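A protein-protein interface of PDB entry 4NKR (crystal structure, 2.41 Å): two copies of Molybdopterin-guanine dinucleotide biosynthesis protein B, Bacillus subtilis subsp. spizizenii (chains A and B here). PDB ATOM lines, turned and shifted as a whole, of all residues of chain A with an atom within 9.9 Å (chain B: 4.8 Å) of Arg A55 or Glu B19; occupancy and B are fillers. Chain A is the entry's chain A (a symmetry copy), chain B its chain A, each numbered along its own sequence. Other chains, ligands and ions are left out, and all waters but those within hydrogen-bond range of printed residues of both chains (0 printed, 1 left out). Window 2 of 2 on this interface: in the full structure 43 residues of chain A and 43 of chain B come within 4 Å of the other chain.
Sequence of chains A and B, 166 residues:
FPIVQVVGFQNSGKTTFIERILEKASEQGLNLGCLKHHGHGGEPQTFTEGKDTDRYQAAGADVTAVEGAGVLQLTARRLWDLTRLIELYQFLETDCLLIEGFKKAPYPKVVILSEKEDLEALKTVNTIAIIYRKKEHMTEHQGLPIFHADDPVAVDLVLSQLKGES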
ATOM      1  N   ASP A  54     -31.240   8.605  22.161  1.00  0.00           N
ATOM      2  CA  ASP A  54     -30.353   8.282  23.275  1.00  0.00           C
ATOM      3  C   ASP A  54     -29.668   6.909  23.101  1.00  0.00           C
ATOM      4  O   ASP A  54     -28.800   6.502  23.895  1.00  0.00           O
ATOM      5  CB  ASP A  54     -31.147   8.354  24.594  1.00  0.00           C
ATOM      6  CG  ASP A  54     -30.299   8.889  25.780  1.00  0.00           C
ATOM      7  OD1 ASP A  54     -29.494   8.101  26.359  1.00  0.00           O
ATOM      8  OD2 ASP A  54     -30.455  10.097  26.122  1.00  0.00           O
ATOM      9  N   ARG A  55     -30.013   6.246  22.014  1.00  0.00           N
ATOM     10  CA  ARG A  55     -29.645   4.869  21.755  1.00  0.00           C
ATOM     11  C   ARG A  55     -28.120   4.710  21.653  1.00  0.00           C
ATOM     12  O   ARG A  55     -27.512   3.841  22.322  1.00  0.00           O
ATOM     13  CB  ARG A  55     -30.302   4.445  20.433  1.00  0.00           C
ATOM     14  CG  ARG A  55     -30.683   2.986  20.336  1.00  0.00           C
ATOM     15  CD  ARG A  55     -32.186   2.793  20.352  1.00  0.00           C
ATOM     16  NE  ARG A  55     -32.781   2.632  19.030  1.00  0.00           N
ATOM     17  CZ  ARG A  55     -32.649   1.552  18.264  1.00  0.00           C
ATOM     18  NH1 ARG A  55     -31.841   0.565  18.625  1.00  0.00           N
ATOM     19  NH2 ARG A  55     -33.265   1.488  17.089  1.00  0.00           N
ATOM     20  N   TYR A  56     -27.507   5.554  20.828  1.00  0.00           N
ATOM     21  CA  TYR A  56     -26.088   5.475  20.556  1.00  0.00           C
ATOM     22  C   TYR A  56     -25.366   5.926  21.818  1.00  0.00           C
ATOM     23  O   TYR A  56     -24.321   5.360  22.218  1.00  0.00           O
ATOM     24  CB  TYR A  56     -25.699   6.377  19.325  1.00  0.00           C
ATOM     25  CG  TYR A  56     -26.327   5.976  17.973  1.00  0.00           C
ATOM     26  CD1 TYR A  56     -26.736   4.697  17.750  1.00  0.00           C
ATOM     27  CD2 TYR A  56     -26.465   6.910  16.916  1.00  0.00           C
ATOM     28  CE1 TYR A  56     -27.309   4.313  16.554  1.00  0.00           C
ATOM     29  CE2 TYR A  56     -27.016   6.540  15.678  1.00  0.00           C
ATOM     30  CZ  TYR A  56     -27.464   5.230  15.508  1.00  0.00           C
ATOM     31  OH  TYR A  56     -28.056   4.759  14.325  1.00  0.00           O
ATOM     32  N   GLN A  57     -25.940   6.934  22.460  1.00  0.00           N
ATOM     33  CA  GLN A  57     -25.440   7.408  23.749  1.00  0.00           C
ATOM     34  C   GLN A  57     -25.517   6.312  24.810  1.00  0.00           C
ATOM     35  O   GLN A  57     -24.600   6.155  25.593  1.00  0.00           O
ATOM     36  CB  GLN A  57     -26.202   8.664  24.202  1.00  0.00           C
ATOM     37  CG  GLN A  57     -25.481   9.490  25.255  1.00  0.00           C
ATOM     38  CD  GLN A  57     -24.146  10.084  24.776  1.00  0.00           C
ATOM     39  OE1 GLN A  57     -24.059  10.705  23.710  1.00  0.00           O
ATOM     40  NE2 GLN A  57     -23.105   9.906  25.578  1.00  0.00           N
ATOM     41  N   ALA A  58     -26.598   5.530  24.794  1.00  0.00           N
ATOM     42  CA  ALA A  58     -26.811   4.444  25.776  1.00  0.00           C
ATOM     43  C   ALA A  58     -25.896   3.229  25.545  1.00  0.00           C
ATOM     44  O   ALA A  58     -25.433   2.581  26.506  1.00  0.00           O
ATOM     45  CB  ALA A  58     -28.275   3.995  25.745  1.00  0.00           C
ATOM     46  N   ALA A  59     -25.678   2.889  24.276  1.00  0.00           N
ATOM     47  CA  ALA A  59     -24.816   1.779  23.937  1.00  0.00           C
ATOM     48  C   ALA A  59     -23.351   2.080  24.264  1.00  0.00           C
ATOM     49  O   ALA A  59     -22.480   1.254  24.071  1.00  0.00           O
ATOM     50  CB  ALA A  59     -24.972   1.439  22.468  1.00  0.00           C
ATOM     51  N   GLY A  60     -23.075   3.280  24.731  1.00  0.00           N
ATOM     52  CA  GLY A  60     -21.779   3.573  25.281  1.00  0.00           C
ATOM     53  C   GLY A  60     -20.934   4.619  24.570  1.00  0.00           C
ATOM     54  O   GLY A  60     -19.831   4.921  25.044  1.00  0.00           O
ATOM     55  N   ALA A  61     -21.406   5.203  23.470  1.00  0.00           N
ATOM     56  CA  ALA A  61     -20.587   6.247  22.852  1.00  0.00           C
ATOM     57  C   ALA A  61     -20.590   7.544  23.696  1.00  0.00           C
ATOM     58  O   ALA A  61     -21.625   7.971  24.202  1.00  0.00           O
ATOM     59  CB  ALA A  61     -21.026   6.525  21.433  1.00  0.00           C
ATOM     60  N   ASP A  62     -19.413   8.134  23.812  1.00  0.00           N
ATOM     61  CA  ASP A  62     -19.133   9.381  24.572  1.00  0.00           C
ATOM     62  C   ASP A  62     -19.429  10.668  23.807  1.00  0.00           C
ATOM     63  O   ASP A  62     -19.864  11.690  24.423  1.00  0.00           O
ATOM     64  CB  ASP A  62     -17.602   9.431  24.925  1.00  0.00           C
ATOM     65  CG  ASP A  62     -16.674   9.126  23.659  1.00  0.00           C
ATOM     66  OD1 ASP A  62     -17.199   8.599  22.617  1.00  0.00           O
ATOM     67  OD2 ASP A  62     -15.437   9.408  23.706  1.00  0.00           O
ATOM     68  N   THR A  64     -21.414  11.785  20.443  1.00  0.00           N
ATOM     69  CA  THR A  64     -22.486  11.402  19.451  1.00  0.00           C
ATOM     70  C   THR A  64     -23.099  12.691  18.861  1.00  0.00           C
ATOM     71  O   THR A  64     -23.229  13.705  19.549  1.00  0.00           O
ATOM     72  CB  THR A  64     -23.734  10.641  20.123  1.00  0.00           C
ATOM     73  OG1 THR A  64     -24.233  11.407  21.193  1.00  0.00           O
ATOM     74  CG2 THR A  64     -23.412   9.268  20.694  1.00  0.00           C
ATOM     75  N   VAL A  66     -25.974  14.381  15.477  1.00  0.00           N
ATOM     76  CA  VAL A  66     -26.813  14.415  14.283  1.00  0.00           C
ATOM     77  C   VAL A  66     -26.605  15.691  13.529  1.00  0.00           C
ATOM     78  O   VAL A  66     -26.576  16.775  14.116  1.00  0.00           O
ATOM     79  CB  VAL A  66     -28.319  14.340  14.602  1.00  0.00           C
ATOM     80  CG1 VAL A  66     -29.092  14.112  13.304  1.00  0.00           C
ATOM     81  CG2 VAL A  66     -28.600  13.157  15.492  1.00  0.00           C
ATOM     82  N   THR A  75     -23.892  15.803  21.383  1.00  0.00           N
ATOM     83  CA  THR A  75     -23.680  15.530  22.823  1.00  0.00           C
ATOM     84  C   THR A  75     -22.254  14.910  23.027  1.00  0.00           C
ATOM     85  O   THR A  75     -21.887  13.928  22.375  1.00  0.00           O
ATOM     86  CB  THR A  75     -24.667  14.505  23.334  1.00  0.00           C
ATOM     87  OG1 THR A  75     -24.493  13.334  22.530  1.00  0.00           O
ATOM     88  CG2 THR A  75     -26.072  14.947  23.154  1.00  0.00           C
ATOM     89  N   THR B  15     -29.535   1.224  12.806  1.00  0.00           N
ATOM     90  CA  THR B  15     -29.369   1.589  14.227  1.00  0.00           C
ATOM     91  C   THR B  15     -28.979   0.387  15.093  1.00  0.00           C
ATOM     92  O   THR B  15     -28.075   0.448  15.940  1.00  0.00           O
ATOM     93  CB  THR B  15     -30.654   2.231  14.732  1.00  0.00           C
ATOM     94  OG1 THR B  15     -31.034   3.288  13.809  1.00  0.00           O
ATOM     95  CG2 THR B  15     -30.484   2.789  16.138  1.00  0.00           C
ATOM     96  N   THR B  16     -29.624  -0.729  14.856  1.00  0.00           N
ATOM     97  CA  THR B  16     -29.295  -1.929  15.573  1.00  0.00           C
ATOM     98  C   THR B  16     -27.887  -2.346  15.294  1.00  0.00           C
ATOM     99  O   THR B  16     -27.109  -2.496  16.181  1.00  0.00           O
ATOM    100  CB  THR B  16     -30.279  -3.058  15.242  1.00  0.00           C
ATOM    101  OG1 THR B  16     -31.380  -2.956  16.130  1.00  0.00           O
ATOM    102  CG2 THR B  16     -29.669  -4.394  15.444  1.00  0.00           C
ATOM    103  N   PHE B  17     -27.542  -2.530  14.051  1.00  0.00           N
ATOM    104  CA  PHE B  17     -26.122  -2.711  13.734  1.00  0.00           C
ATOM    105  C   PHE B  17     -25.159  -1.745  14.453  1.00  0.00           C
ATOM    106  O   PHE B  17     -24.191  -2.179  15.071  1.00  0.00           O
ATOM    107  CB  PHE B  17     -25.891  -2.632  12.239  1.00  0.00           C
ATOM    108  CG  PHE B  17     -24.602  -3.183  11.828  1.00  0.00           C
ATOM    109  CD1 PHE B  17     -24.234  -4.441  12.217  1.00  0.00           C
ATOM    110  CD2 PHE B  17     -23.707  -2.417  11.034  1.00  0.00           C
ATOM    111  CE1 PHE B  17     -23.006  -4.956  11.834  1.00  0.00           C
ATOM    112  CE2 PHE B  17     -22.526  -2.944  10.606  1.00  0.00           C
ATOM    113  CZ  PHE B  17     -22.158  -4.201  11.011  1.00  0.00           C
ATOM    114  N   ILE B  18     -25.432  -0.450  14.382  1.00  0.00           N
ATOM    115  CA  ILE B  18     -24.594   0.524  15.035  1.00  0.00           C
ATOM    116  C   ILE B  18     -24.537   0.344  16.530  1.00  0.00           C
ATOM    117  O   ILE B  18     -23.483   0.526  17.145  1.00  0.00           O
ATOM    118  CB  ILE B  18     -24.988   1.950  14.620  1.00  0.00           C
ATOM    119  CG1 ILE B  18     -24.340   2.294  13.252  1.00  0.00           C
ATOM    120  CG2 ILE B  18     -24.526   3.000  15.631  1.00  0.00           C
ATOM    121  CD1 ILE B  18     -25.323   2.933  12.281  1.00  0.00           C
ATOM    122  N   GLU B  19     -25.663  -0.015  17.130  1.00  0.00           N
ATOM    123  CA  GLU B  19     -25.734  -0.208  18.586  1.00  0.00           C
ATOM    124  C   GLU B  19     -24.831  -1.330  19.036  1.00  0.00           C
ATOM    125  O   GLU B  19     -24.146  -1.212  20.048  1.00  0.00           O
ATOM    126  CB  GLU B  19     -27.167  -0.565  19.017  1.00  0.00           C
ATOM    127  CG  GLU B  19     -28.016   0.585  19.507  1.00  0.00           C
ATOM    128  CD  GLU B  19     -29.185   0.071  20.358  1.00  0.00           C
ATOM    129  OE1 GLU B  19     -29.921  -0.810  19.838  1.00  0.00           O
ATOM    130  OE2 GLU B  19     -29.356   0.511  21.545  1.00  0.00           O
ATOM    131  N   ARG B  20     -24.890  -2.453  18.333  1.00  0.00           N
ATOM    132  CA  ARG B  20     -24.018  -3.577  18.611  1.00  0.00           C
ATOM    133  C   ARG B  20     -22.548  -3.186  18.529  1.00  0.00           C
ATOM    134  O   ARG B  20     -21.762  -3.470  19.432  1.00  0.00           O
ATOM    135  CB  ARG B  20     -24.308  -4.762  17.685  1.00  0.00           C
ATOM    136  CG  ARG B  20     -25.644  -5.443  17.938  1.00  0.00           C
ATOM    137  CD  ARG B  20     -25.918  -6.601  16.962  1.00  0.00           C
ATOM    138  NE  ARG B  20     -27.287  -7.122  17.106  1.00  0.00           N
ATOM    139  CZ  ARG B  20     -27.833  -8.038  16.315  1.00  0.00           C
ATOM    140  NH1 ARG B  20     -27.131  -8.560  15.325  1.00  0.00           N
ATOM    141  NH2 ARG B  20     -29.089  -8.431  16.513  1.00  0.00           N
ATOM    142  N   ILE B  21     -22.182  -2.459  17.504  1.00  0.00           N
ATOM    143  CA  ILE B  21     -20.804  -1.984  17.393  1.00  0.00           C
ATOM    144  C   ILE B  21     -20.397  -1.073  18.536  1.00  0.00           C
ATOM    145  O   ILE B  21     -19.268  -1.163  19.054  1.00  0.00           O
ATOM    146  CB  ILE B  21     -20.605  -1.170  16.118  1.00  0.00           C
ATOM    147  CG1 ILE B  21     -20.889  -2.029  14.886  1.00  0.00           C
ATOM    148  CG2 ILE B  21     -19.200  -0.601  16.085  1.00  0.00           C
ATOM    149  CD1 ILE B  21     -21.067  -1.209  13.634  1.00  0.00           C
ATOM    150  N   LEU B  22     -21.242  -0.104  18.853  1.00  0.00           N
ATOM    151  CA  LEU B  22     -20.904   0.808  19.947  1.00  0.00           C
ATOM    152  C   LEU B  22     -20.787   0.091  21.315  1.00  0.00           C
ATOM    153  O   LEU B  22     -19.827   0.354  22.065  1.00  0.00           O
ATOM    154  CB  LEU B  22     -21.881   1.946  20.028  1.00  0.00           C
ATOM    155  CG  LEU B  22     -21.866   2.871  18.835  1.00  0.00           C
ATOM    156  CD1 LEU B  22     -22.958   3.925  18.943  1.00  0.00           C
ATOM    157  CD2 LEU B  22     -20.488   3.524  18.694  1.00  0.00           C
ATOM    158  N   GLU B  23     -21.709  -0.836  21.604  1.00  0.00           N
ATOM    159  CA  GLU B  23     -21.696  -1.615  22.873  1.00  0.00           C
ATOM    160  C   GLU B  23     -20.377  -2.374  22.993  1.00  0.00           C
ATOM    161  O   GLU B  23     -19.630  -2.239  23.970  1.00  0.00           O
ATOM    162  CB  GLU B  23     -22.890  -2.596  22.939  1.00  0.00           C
ATOM    163  CG  GLU B  23     -24.242  -1.892  23.164  1.00  0.00           C
ATOM    164  CD  GLU B  23     -25.493  -2.724  22.824  1.00  0.00           C
ATOM    165  OE1 GLU B  23     -26.526  -2.555  23.515  1.00  0.00           O
ATOM    166  OE2 GLU B  23     -25.475  -3.514  21.859  1.00  0.00           O
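No position is printed for both chains. Of the 8 pairs that touch across the chains among the printed residues, none has its exchanged pair printed and touching as well.
Arg A55 touches Thr B15 (NH2 to CG2, 3.2 Å). CG2 of Ile B18 touches CE1 of Tyr A56, at 3.2 Å. Tyr A56 touches Leu B22. CB of Ala A59 touches O of Glu B19, 3.7 Å away.
The backbone carbonyl oxygen of Tyr A56 lies within hydrogen-bond range of the backbone NH of Ala A61 (3.2 Å).
Of chain B, only Thr B15 (3.2 Å) and Glu B19 (2.7 Å) come within 4 Å of Arg A55. Printed residues of chain B within 4 Å of Ala A59: Glu B19 (3.7 Å), Leu B22 (3.4 Å) and Glu B23 (3.2 Å). Of chain A, only Arg A55 (3.2 Å) and Tyr A56 (3.4 Å) come within 4 Å of Thr B15. Phe B17 touches none of the printed residues of chain A. Of chain A, only Arg A55 and Ala A59 come within 4 Å of Glu B19. Of the printed residues of chain A, Glu B23 touches Ala A59 (3.2 Å). The nearest residue of chain B that does not touch Arg A55 is Thr B16 (4.3 Å). The nearest residue of chain A that does not touch Glu B19 is Tyr A56 (4.7 Å).
OH of Tyr A56 lies within hydrogen-bond range of OG1 of Thr B15. OE1 of Glu B19 lies within salt-bridge range of NH1 of Arg A55. O of Ala A59 sits close to N of Glu B23 (3.3 Å). O of Leu B22 sits close to O of Ala A59 (3.4 Å).
Of the 9 printed residues of chain B, 5 touch a printed residue of chain A. Printed residues of chain B that touch a printed residue of chain A: Thr B15, Ile B18, Glu B19, Leu B22 and Glu B23. Of the 12 printed residues of chain A, 3 touch a printed residue of chain B. Printed residues of chain A that touch a printed residue of chain B: Arg A55, Tyr A56 and Ala A59. Among the printed residues, Asp or Glu carboxylates within 4 Å of a Lys or Arg side-chain nitrogen of the other chain: Arg A55 with Glu B19.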
